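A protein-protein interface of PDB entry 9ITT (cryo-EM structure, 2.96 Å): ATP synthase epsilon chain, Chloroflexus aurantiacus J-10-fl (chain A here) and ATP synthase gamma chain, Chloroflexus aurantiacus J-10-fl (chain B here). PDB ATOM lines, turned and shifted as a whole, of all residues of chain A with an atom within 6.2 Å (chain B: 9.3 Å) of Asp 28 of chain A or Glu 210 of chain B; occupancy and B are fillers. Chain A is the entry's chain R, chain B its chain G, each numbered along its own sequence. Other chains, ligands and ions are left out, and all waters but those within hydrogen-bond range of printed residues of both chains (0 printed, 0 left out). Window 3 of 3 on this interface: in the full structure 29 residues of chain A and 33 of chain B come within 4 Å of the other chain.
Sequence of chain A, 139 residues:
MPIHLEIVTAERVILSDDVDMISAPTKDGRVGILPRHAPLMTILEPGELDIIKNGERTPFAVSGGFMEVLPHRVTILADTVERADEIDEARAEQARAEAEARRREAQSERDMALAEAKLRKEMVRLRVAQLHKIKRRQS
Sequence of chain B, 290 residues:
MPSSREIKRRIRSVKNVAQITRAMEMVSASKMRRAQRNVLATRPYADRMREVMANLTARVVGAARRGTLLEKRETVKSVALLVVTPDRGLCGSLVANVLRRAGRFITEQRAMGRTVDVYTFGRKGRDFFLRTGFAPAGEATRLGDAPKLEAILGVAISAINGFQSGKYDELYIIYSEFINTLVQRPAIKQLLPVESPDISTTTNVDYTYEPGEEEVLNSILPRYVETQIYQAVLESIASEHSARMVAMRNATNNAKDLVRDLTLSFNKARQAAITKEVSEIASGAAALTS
Asp 28 of chain A touches just one residue of chain B: Glu 210. Gly 29 of chain A touches none of the printed residues of chain B. Printed residues of chain B within 4 Å of Leu 40 of chain A: Thr 208 and Glu 210. Of the printed residues of chain B, Ile 43 of chain A touches Pro 211 (3.6 Å), Glu 215 (3.8 Å) and Val 216 (3.9 Å). Of the printed residues of chain A, Tyr 209 of chain B touches Met 41. Glu 210 of chain B touches three residues of chain A. Of the printed residues of chain A, Glu 215 of chain B touches Ile 43 (3.8 Å). Printed residues of chain A within 4 Å of Val 216 of chain B: Ile 43. The nearest residue of chain B that does not touch Asp 28 of chain A is Pro 211 of chain B (4.7 Å). The nearest residue of chain A that does not touch Glu 210 of chain B is Thr 26 of chain A (4.4 Å).
N of Lys 27 of chain A lies within hydrogen-bond range of O of Ile 43 of chain A (2.7 Å).
CA of Leu 40 of chain A touches O of Thr 208 of chain B, at 3.3 Å. Leu 40 of chain A touches Glu 210 of chain B (CD1 to CG, 3.9 Å). Tyr 207 of chain B touches Met 41 of chain A. Met 41 of chain A touches Tyr 209 of chain B. Ile 43 of chain A touches Pro 211 of chain B (CG1 to CG, 3.6 Å). CG of Glu 215 of chain B touches CD1 of Ile 43 of chain A, at 3.8 Å. Ile 43 of chain A touches Val 216 of chain B.
The backbone carbonyl oxygen (O) of Thr 208 of chain B sits at hydrogen-bond distance from the backbone NH (N) of Met 41 of chain A, 2.8 Å away. The backbone NH (N) of Glu 210 of chain B lies within hydrogen-bond range of the backbone carbonyl oxygen (O) of Met 41 of chain A (3.4 Å). The side-chain carboxylate (OD2) of Asp 28 of chain A sits close to the side-chain carboxylate (OE1) of Glu 210 of chain B.
Of the 10 printed residues of chain B, 7 touch a printed residue of chain A. Hydrophobic or aromatic side chains of chain B within 4 Å of the printed part of chain A: Tyr 207, Tyr 209, Pro 211 and Val 216. Hydrophobic or aromatic side chains of chain A that line the printed part of chain B: Leu 40, Met 41 and Ile 43. Among the printed residues, 10 pairs touch across the chains.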
ATOM      1  N   THR A  26      18.784   4.342  -6.774  1.00  0.00           N
ATOM      2  CA  THR A  26      20.090   4.810  -7.214  1.00  0.00           C
ATOM      3  C   THR A  26      19.968   6.153  -7.932  1.00  0.00           C
ATOM      4  O   THR A  26      18.914   6.503  -8.470  1.00  0.00           O
ATOM      5  CB  THR A  26      20.736   3.756  -8.121  1.00  0.00           C
ATOM      6  OG1 THR A  26      21.065   2.597  -7.344  1.00  0.00           O
ATOM      7  CG2 THR A  26      21.999   4.275  -8.806  1.00  0.00           C
ATOM      8  N   LYS A  27      21.067   6.918  -7.912  1.00  0.00           N
ATOM      9  CA  LYS A  27      21.096   8.234  -8.544  1.00  0.00           C
ATOM     10  C   LYS A  27      20.684   8.172 -10.011  1.00  0.00           C
ATOM     11  O   LYS A  27      19.803   8.923 -10.446  1.00  0.00           O
ATOM     12  CB  LYS A  27      22.497   8.836  -8.418  1.00  0.00           C
ATOM     13  CG  LYS A  27      22.695   9.707  -7.186  1.00  0.00           C
ATOM     14  CD  LYS A  27      23.950  10.556  -7.291  1.00  0.00           C
ATOM     15  CE  LYS A  27      24.054  11.528  -6.127  1.00  0.00           C
ATOM     16  NZ  LYS A  27      25.352  12.255  -6.116  1.00  0.00           N
ATOM     17  N   ASP A  28      21.309   7.289 -10.793  1.00  0.00           N
ATOM     18  CA  ASP A  28      20.990   7.217 -12.216  1.00  0.00           C
ATOM     19  C   ASP A  28      19.552   6.774 -12.458  1.00  0.00           C
ATOM     20  O   ASP A  28      18.965   7.121 -13.488  1.00  0.00           O
ATOM     21  CB  ASP A  28      21.973   6.283 -12.934  1.00  0.00           C
ATOM     22  CG  ASP A  28      21.831   4.815 -12.526  1.00  0.00           C
ATOM     23  OD1 ASP A  28      20.944   4.463 -11.722  1.00  0.00           O
ATOM     24  OD2 ASP A  28      22.632   3.998 -13.025  1.00  0.00           O
ATOM     25  N   GLY A  29      18.984   6.014 -11.537  1.00  0.00           N
ATOM     26  CA  GLY A  29      17.613   5.562 -11.646  1.00  0.00           C
ATOM     27  C   GLY A  29      17.366   4.377 -10.748  1.00  0.00           C
ATOM     28  O   GLY A  29      18.285   3.671 -10.336  1.00  0.00           O
ATOM     29  N   ARG A  30      16.089   4.156 -10.449  1.00  0.00           N
ATOM     30  CA  ARG A  30      15.705   3.112  -9.507  1.00  0.00           C
ATOM     31  C   ARG A  30      16.187   1.749  -9.987  1.00  0.00           C
ATOM     32  O   ARG A  30      16.113   1.434 -11.178  1.00  0.00           O
ATOM     33  CB  ARG A  30      14.190   3.097  -9.324  1.00  0.00           C
ATOM     34  CG  ARG A  30      13.645   4.335  -8.642  1.00  0.00           C
ATOM     35  CD  ARG A  30      12.201   4.143  -8.220  1.00  0.00           C
ATOM     36  NE  ARG A  30      11.726   5.245  -7.393  1.00  0.00           N
ATOM     37  CZ  ARG A  30      10.500   5.340  -6.893  1.00  0.00           C
ATOM     38  NH1 ARG A  30       9.584   4.411  -7.118  1.00  0.00           N
ATOM     39  NH2 ARG A  30      10.185   6.395  -6.148  1.00  0.00           N
ATOM     40  N   VAL A  31      16.689   0.946  -9.050  1.00  0.00           N
ATOM     41  CA  VAL A  31      17.195  -0.390  -9.330  1.00  0.00           C
ATOM     42  C   VAL A  31      16.544  -1.364  -8.357  1.00  0.00           C
ATOM     43  O   VAL A  31      16.178  -1.001  -7.235  1.00  0.00           O
ATOM     44  CB  VAL A  31      18.737  -0.452  -9.224  1.00  0.00           C
ATOM     45  CG1 VAL A  31      19.264  -1.845  -9.566  1.00  0.00           C
ATOM     46  CG2 VAL A  31      19.370   0.590 -10.131  1.00  0.00           C
ATOM     47  N   LEU A  40      28.118  -4.831  -6.887  1.00  0.00           N
ATOM     48  CA  LEU A  40      27.697  -3.498  -7.315  1.00  0.00           C
ATOM     49  C   LEU A  40      27.836  -2.528  -6.155  1.00  0.00           C
ATOM     50  O   LEU A  40      27.550  -2.889  -5.009  1.00  0.00           O
ATOM     51  CB  LEU A  40      26.251  -3.538  -7.822  1.00  0.00           C
ATOM     52  CG  LEU A  40      25.575  -2.215  -8.205  1.00  0.00           C
ATOM     53  CD1 LEU A  40      24.582  -2.444  -9.333  1.00  0.00           C
ATOM     54  CD2 LEU A  40      24.863  -1.563  -7.018  1.00  0.00           C
ATOM     55  N   MET A  41      28.276  -1.308  -6.451  1.00  0.00           N
ATOM     56  CA  MET A  41      28.211  -0.178  -5.536  1.00  0.00           C
ATOM     57  C   MET A  41      27.452   0.961  -6.200  1.00  0.00           C
ATOM     58  O   MET A  41      27.469   1.118  -7.423  1.00  0.00           O
ATOM     59  CB  MET A  41      29.604   0.300  -5.122  1.00  0.00           C
ATOM     60  CG  MET A  41      30.363  -0.695  -4.283  1.00  0.00           C
ATOM     61  SD  MET A  41      31.942  -0.060  -3.700  1.00  0.00           S
ATOM     62  CE  MET A  41      32.589  -1.501  -2.862  1.00  0.00           C
ATOM     63  N   THR A  42      26.785   1.762  -5.376  1.00  0.00           N
ATOM     64  CA  THR A  42      25.832   2.722  -5.905  1.00  0.00           C
ATOM     65  C   THR A  42      25.564   3.815  -4.884  1.00  0.00           C
ATOM     66  O   THR A  42      25.801   3.637  -3.687  1.00  0.00           O
ATOM     67  CB  THR A  42      24.527   2.021  -6.297  1.00  0.00           C
ATOM     68  OG1 THR A  42      23.652   2.955  -6.926  1.00  0.00           O
ATOM     69  CG2 THR A  42      23.835   1.416  -5.083  1.00  0.00           C
ATOM     70  N   ILE A  43      25.061   4.943  -5.380  1.00  0.00           N
ATOM     71  CA  ILE A  43      24.688   6.093  -4.562  1.00  0.00           C
ATOM     72  C   ILE A  43      23.174   6.224  -4.622  1.00  0.00           C
ATOM     73  O   ILE A  43      22.605   6.435  -5.701  1.00  0.00           O
ATOM     74  CB  ILE A  43      25.367   7.385  -5.042  1.00  0.00           C
ATOM     75  CG1 ILE A  43      26.860   7.163  -5.314  1.00  0.00           C
ATOM     76  CG2 ILE A  43      25.187   8.497  -4.008  1.00  0.00           C
ATOM     77  CD1 ILE A  43      27.565   8.386  -5.860  1.00  0.00           C
ATOM     78  N   GLU A  45      19.366   7.949  -3.466  1.00  0.00           N
ATOM     79  CA  GLU A  45      18.814   9.299  -3.431  1.00  0.00           C
ATOM     80  C   GLU A  45      17.619   9.360  -2.487  1.00  0.00           C
ATOM     81  O   GLU A  45      17.159   8.318  -2.003  1.00  0.00           O
ATOM     82  CB  GLU A  45      18.386   9.752  -4.827  1.00  0.00           C
ATOM     83  CG  GLU A  45      19.507  10.292  -5.688  1.00  0.00           C
ATOM     84  CD  GLU A  45      19.000  10.864  -6.998  1.00  0.00           C
ATOM     85  OE1 GLU A  45      17.776  10.808  -7.238  1.00  0.00           O
ATOM     86  OE2 GLU A  45      19.824  11.371  -7.788  1.00  0.00           O
ATOM     87  N   TYR B 207      33.750  -5.191  -9.096  1.00  0.00           N
ATOM     88  CA  TYR B 207      32.529  -4.465  -8.784  1.00  0.00           C
ATOM     89  C   TYR B 207      32.008  -3.733 -10.013  1.00  0.00           C
ATOM     90  O   TYR B 207      32.666  -3.682 -11.055  1.00  0.00           O
ATOM     91  CB  TYR B 207      32.780  -3.456  -7.659  1.00  0.00           C
ATOM     92  CG  TYR B 207      32.958  -4.069  -6.288  1.00  0.00           C
ATOM     93  CD1 TYR B 207      32.001  -4.919  -5.753  1.00  0.00           C
ATOM     94  CD2 TYR B 207      34.094  -3.808  -5.537  1.00  0.00           C
ATOM     95  CE1 TYR B 207      32.164  -5.480  -4.504  1.00  0.00           C
ATOM     96  CE2 TYR B 207      34.268  -4.367  -4.288  1.00  0.00           C
ATOM     97  CZ  TYR B 207      33.299  -5.202  -3.775  1.00  0.00           C
ATOM     98  OH  TYR B 207      33.466  -5.763  -2.531  1.00  0.00           O
ATOM     99  N   THR B 208      30.810  -3.170  -9.873  1.00  0.00           N
ATOM    100  CA  THR B 208      30.207  -2.311 -10.882  1.00  0.00           C
ATOM    101  C   THR B 208      29.724  -1.043 -10.199  1.00  0.00           C
ATOM    102  O   THR B 208      29.010  -1.110  -9.194  1.00  0.00           O
ATOM    103  CB  THR B 208      29.043  -3.011 -11.590  1.00  0.00           C
ATOM    104  OG1 THR B 208      29.462  -4.307 -12.033  1.00  0.00           O
ATOM    105  CG2 THR B 208      28.577  -2.194 -12.788  1.00  0.00           C
ATOM    106  N   TYR B 209      30.110   0.106 -10.747  1.00  0.00           N
ATOM    107  CA  TYR B 209      29.851   1.409 -10.144  1.00  0.00           C
ATOM    108  C   TYR B 209      28.893   2.162 -11.056  1.00  0.00           C
ATOM    109  O   TYR B 209      29.318   2.758 -12.052  1.00  0.00           O
ATOM    110  CB  TYR B 209      31.160   2.172  -9.947  1.00  0.00           C
ATOM    111  CG  TYR B 209      32.187   1.408  -9.134  1.00  0.00           C
ATOM    112  CD1 TYR B 209      31.798   0.552  -8.114  1.00  0.00           C
ATOM    113  CD2 TYR B 209      33.541   1.525  -9.401  1.00  0.00           C
ATOM    114  CE1 TYR B 209      32.726  -0.148  -7.374  1.00  0.00           C
ATOM    115  CE2 TYR B 209      34.478   0.824  -8.666  1.00  0.00           C
ATOM    116  CZ  TYR B 209      34.064  -0.012  -7.655  1.00  0.00           C
ATOM    117  OH  TYR B 209      34.991  -0.713  -6.919  1.00  0.00           O
ATOM    118  N   GLU B 210      27.607   2.138 -10.714  1.00  0.00           N
ATOM    119  CA  GLU B 210      26.572   2.618 -11.622  1.00  0.00           C
ATOM    120  C   GLU B 210      26.694   4.121 -11.859  1.00  0.00           C
ATOM    121  O   GLU B 210      26.826   4.542 -13.014  1.00  0.00           O
ATOM    122  CB  GLU B 210      25.181   2.249 -11.090  1.00  0.00           C
ATOM    123  CG  GLU B 210      24.743   0.817 -11.391  1.00  0.00           C
ATOM    124  CD  GLU B 210      24.592   0.539 -12.873  1.00  0.00           C
ATOM    125  OE1 GLU B 210      24.213   1.467 -13.619  1.00  0.00           O
ATOM    126  OE2 GLU B 210      24.849  -0.610 -13.293  1.00  0.00           O
ATOM    127  N   PRO B 211      26.655   4.971 -10.823  1.00  0.00           N
ATOM    128  CA  PRO B 211      26.873   6.406 -11.069  1.00  0.00           C
ATOM    129  C   PRO B 211      28.269   6.727 -11.570  1.00  0.00           C
ATOM    130  O   PRO B 211      28.463   7.802 -12.152  1.00  0.00           O
ATOM    131  CB  PRO B 211      26.608   7.055  -9.703  1.00  0.00           C
ATOM    132  CG  PRO B 211      26.635   5.956  -8.722  1.00  0.00           C
ATOM    133  CD  PRO B 211      26.245   4.714  -9.433  1.00  0.00           C
ATOM    134  N   GLY B 212      29.238   5.841 -11.363  1.00  0.00           N
ATOM    135  CA  GLY B 212      30.597   6.042 -11.836  1.00  0.00           C
ATOM    136  C   GLY B 212      31.599   5.854 -10.714  1.00  0.00           C
ATOM    137  O   GLY B 212      31.342   6.187  -9.555  1.00  0.00           O
ATOM    138  N   GLU B 213      32.764   5.308 -11.067  1.00  0.00           N
ATOM    139  CA  GLU B 213      33.804   5.080 -10.070  1.00  0.00           C
ATOM    140  C   GLU B 213      34.252   6.387  -9.431  1.00  0.00           C
ATOM    141  O   GLU B 213      34.360   6.481  -8.203  1.00  0.00           O
ATOM    142  CB  GLU B 213      34.994   4.370 -10.712  1.00  0.00           C
ATOM    143  CG  GLU B 213      36.000   3.813  -9.705  1.00  0.00           C
ATOM    144  CD  GLU B 213      36.789   2.620 -10.228  1.00  0.00           C
ATOM    145  OE1 GLU B 213      36.443   2.076 -11.298  1.00  0.00           O
ATOM    146  OE2 GLU B 213      37.757   2.214  -9.553  1.00  0.00           O
ATOM    147  N   GLU B 214      34.510   7.410 -10.249  1.00  0.00           N
ATOM    148  CA  GLU B 214      34.943   8.693  -9.706  1.00  0.00           C
ATOM    149  C   GLU B 214      33.849   9.338  -8.861  1.00  0.00           C
ATOM    150  O   GLU B 214      34.134   9.917  -7.807  1.00  0.00           O
ATOM    151  CB  GLU B 214      35.397   9.624 -10.838  1.00  0.00           C
ATOM    152  CG  GLU B 214      34.366   9.938 -11.933  1.00  0.00           C
ATOM    153  CD  GLU B 214      34.400   8.949 -13.089  1.00  0.00           C
ATOM    154  OE1 GLU B 214      34.958   7.845 -12.920  1.00  0.00           O
ATOM    155  OE2 GLU B 214      33.868   9.279 -14.170  1.00  0.00           O
ATOM    156  N   GLU B 215      32.589   9.235  -9.291  1.00  0.00           N
ATOM    157  CA  GLU B 215      31.503   9.827  -8.516  1.00  0.00           C
ATOM    158  C   GLU B 215      31.305   9.090  -7.196  1.00  0.00           C
ATOM    159  O   GLU B 215      31.114   9.721  -6.149  1.00  0.00           O
ATOM    160  CB  GLU B 215      30.215   9.822  -9.341  1.00  0.00           C
ATOM    161  CG  GLU B 215      28.993  10.443  -8.658  1.00  0.00           C
ATOM    162  CD  GLU B 215      29.291  11.755  -7.952  1.00  0.00           C
ATOM    163  OE1 GLU B 215      29.318  12.804  -8.630  1.00  0.00           O
ATOM    164  OE2 GLU B 215      29.492  11.739  -6.721  1.00  0.00           O
ATOM    165  N   VAL B 216      31.355   7.756  -7.223  1.00  0.00           N
ATOM    166  CA  VAL B 216      31.234   6.985  -5.990  1.00  0.00           C
ATOM    167  C   VAL B 216      32.378   7.324  -5.045  1.00  0.00           C
ATOM    168  O   VAL B 216      32.185   7.452  -3.832  1.00  0.00           O
ATOM    169  CB  VAL B 216      31.184   5.477  -6.305  1.00  0.00           C
ATOM    170  CG1 VAL B 216      31.407   4.649  -5.046  1.00  0.00           C
ATOM    171  CG2 VAL B 216      29.859   5.118  -6.947  1.00  0.00           C
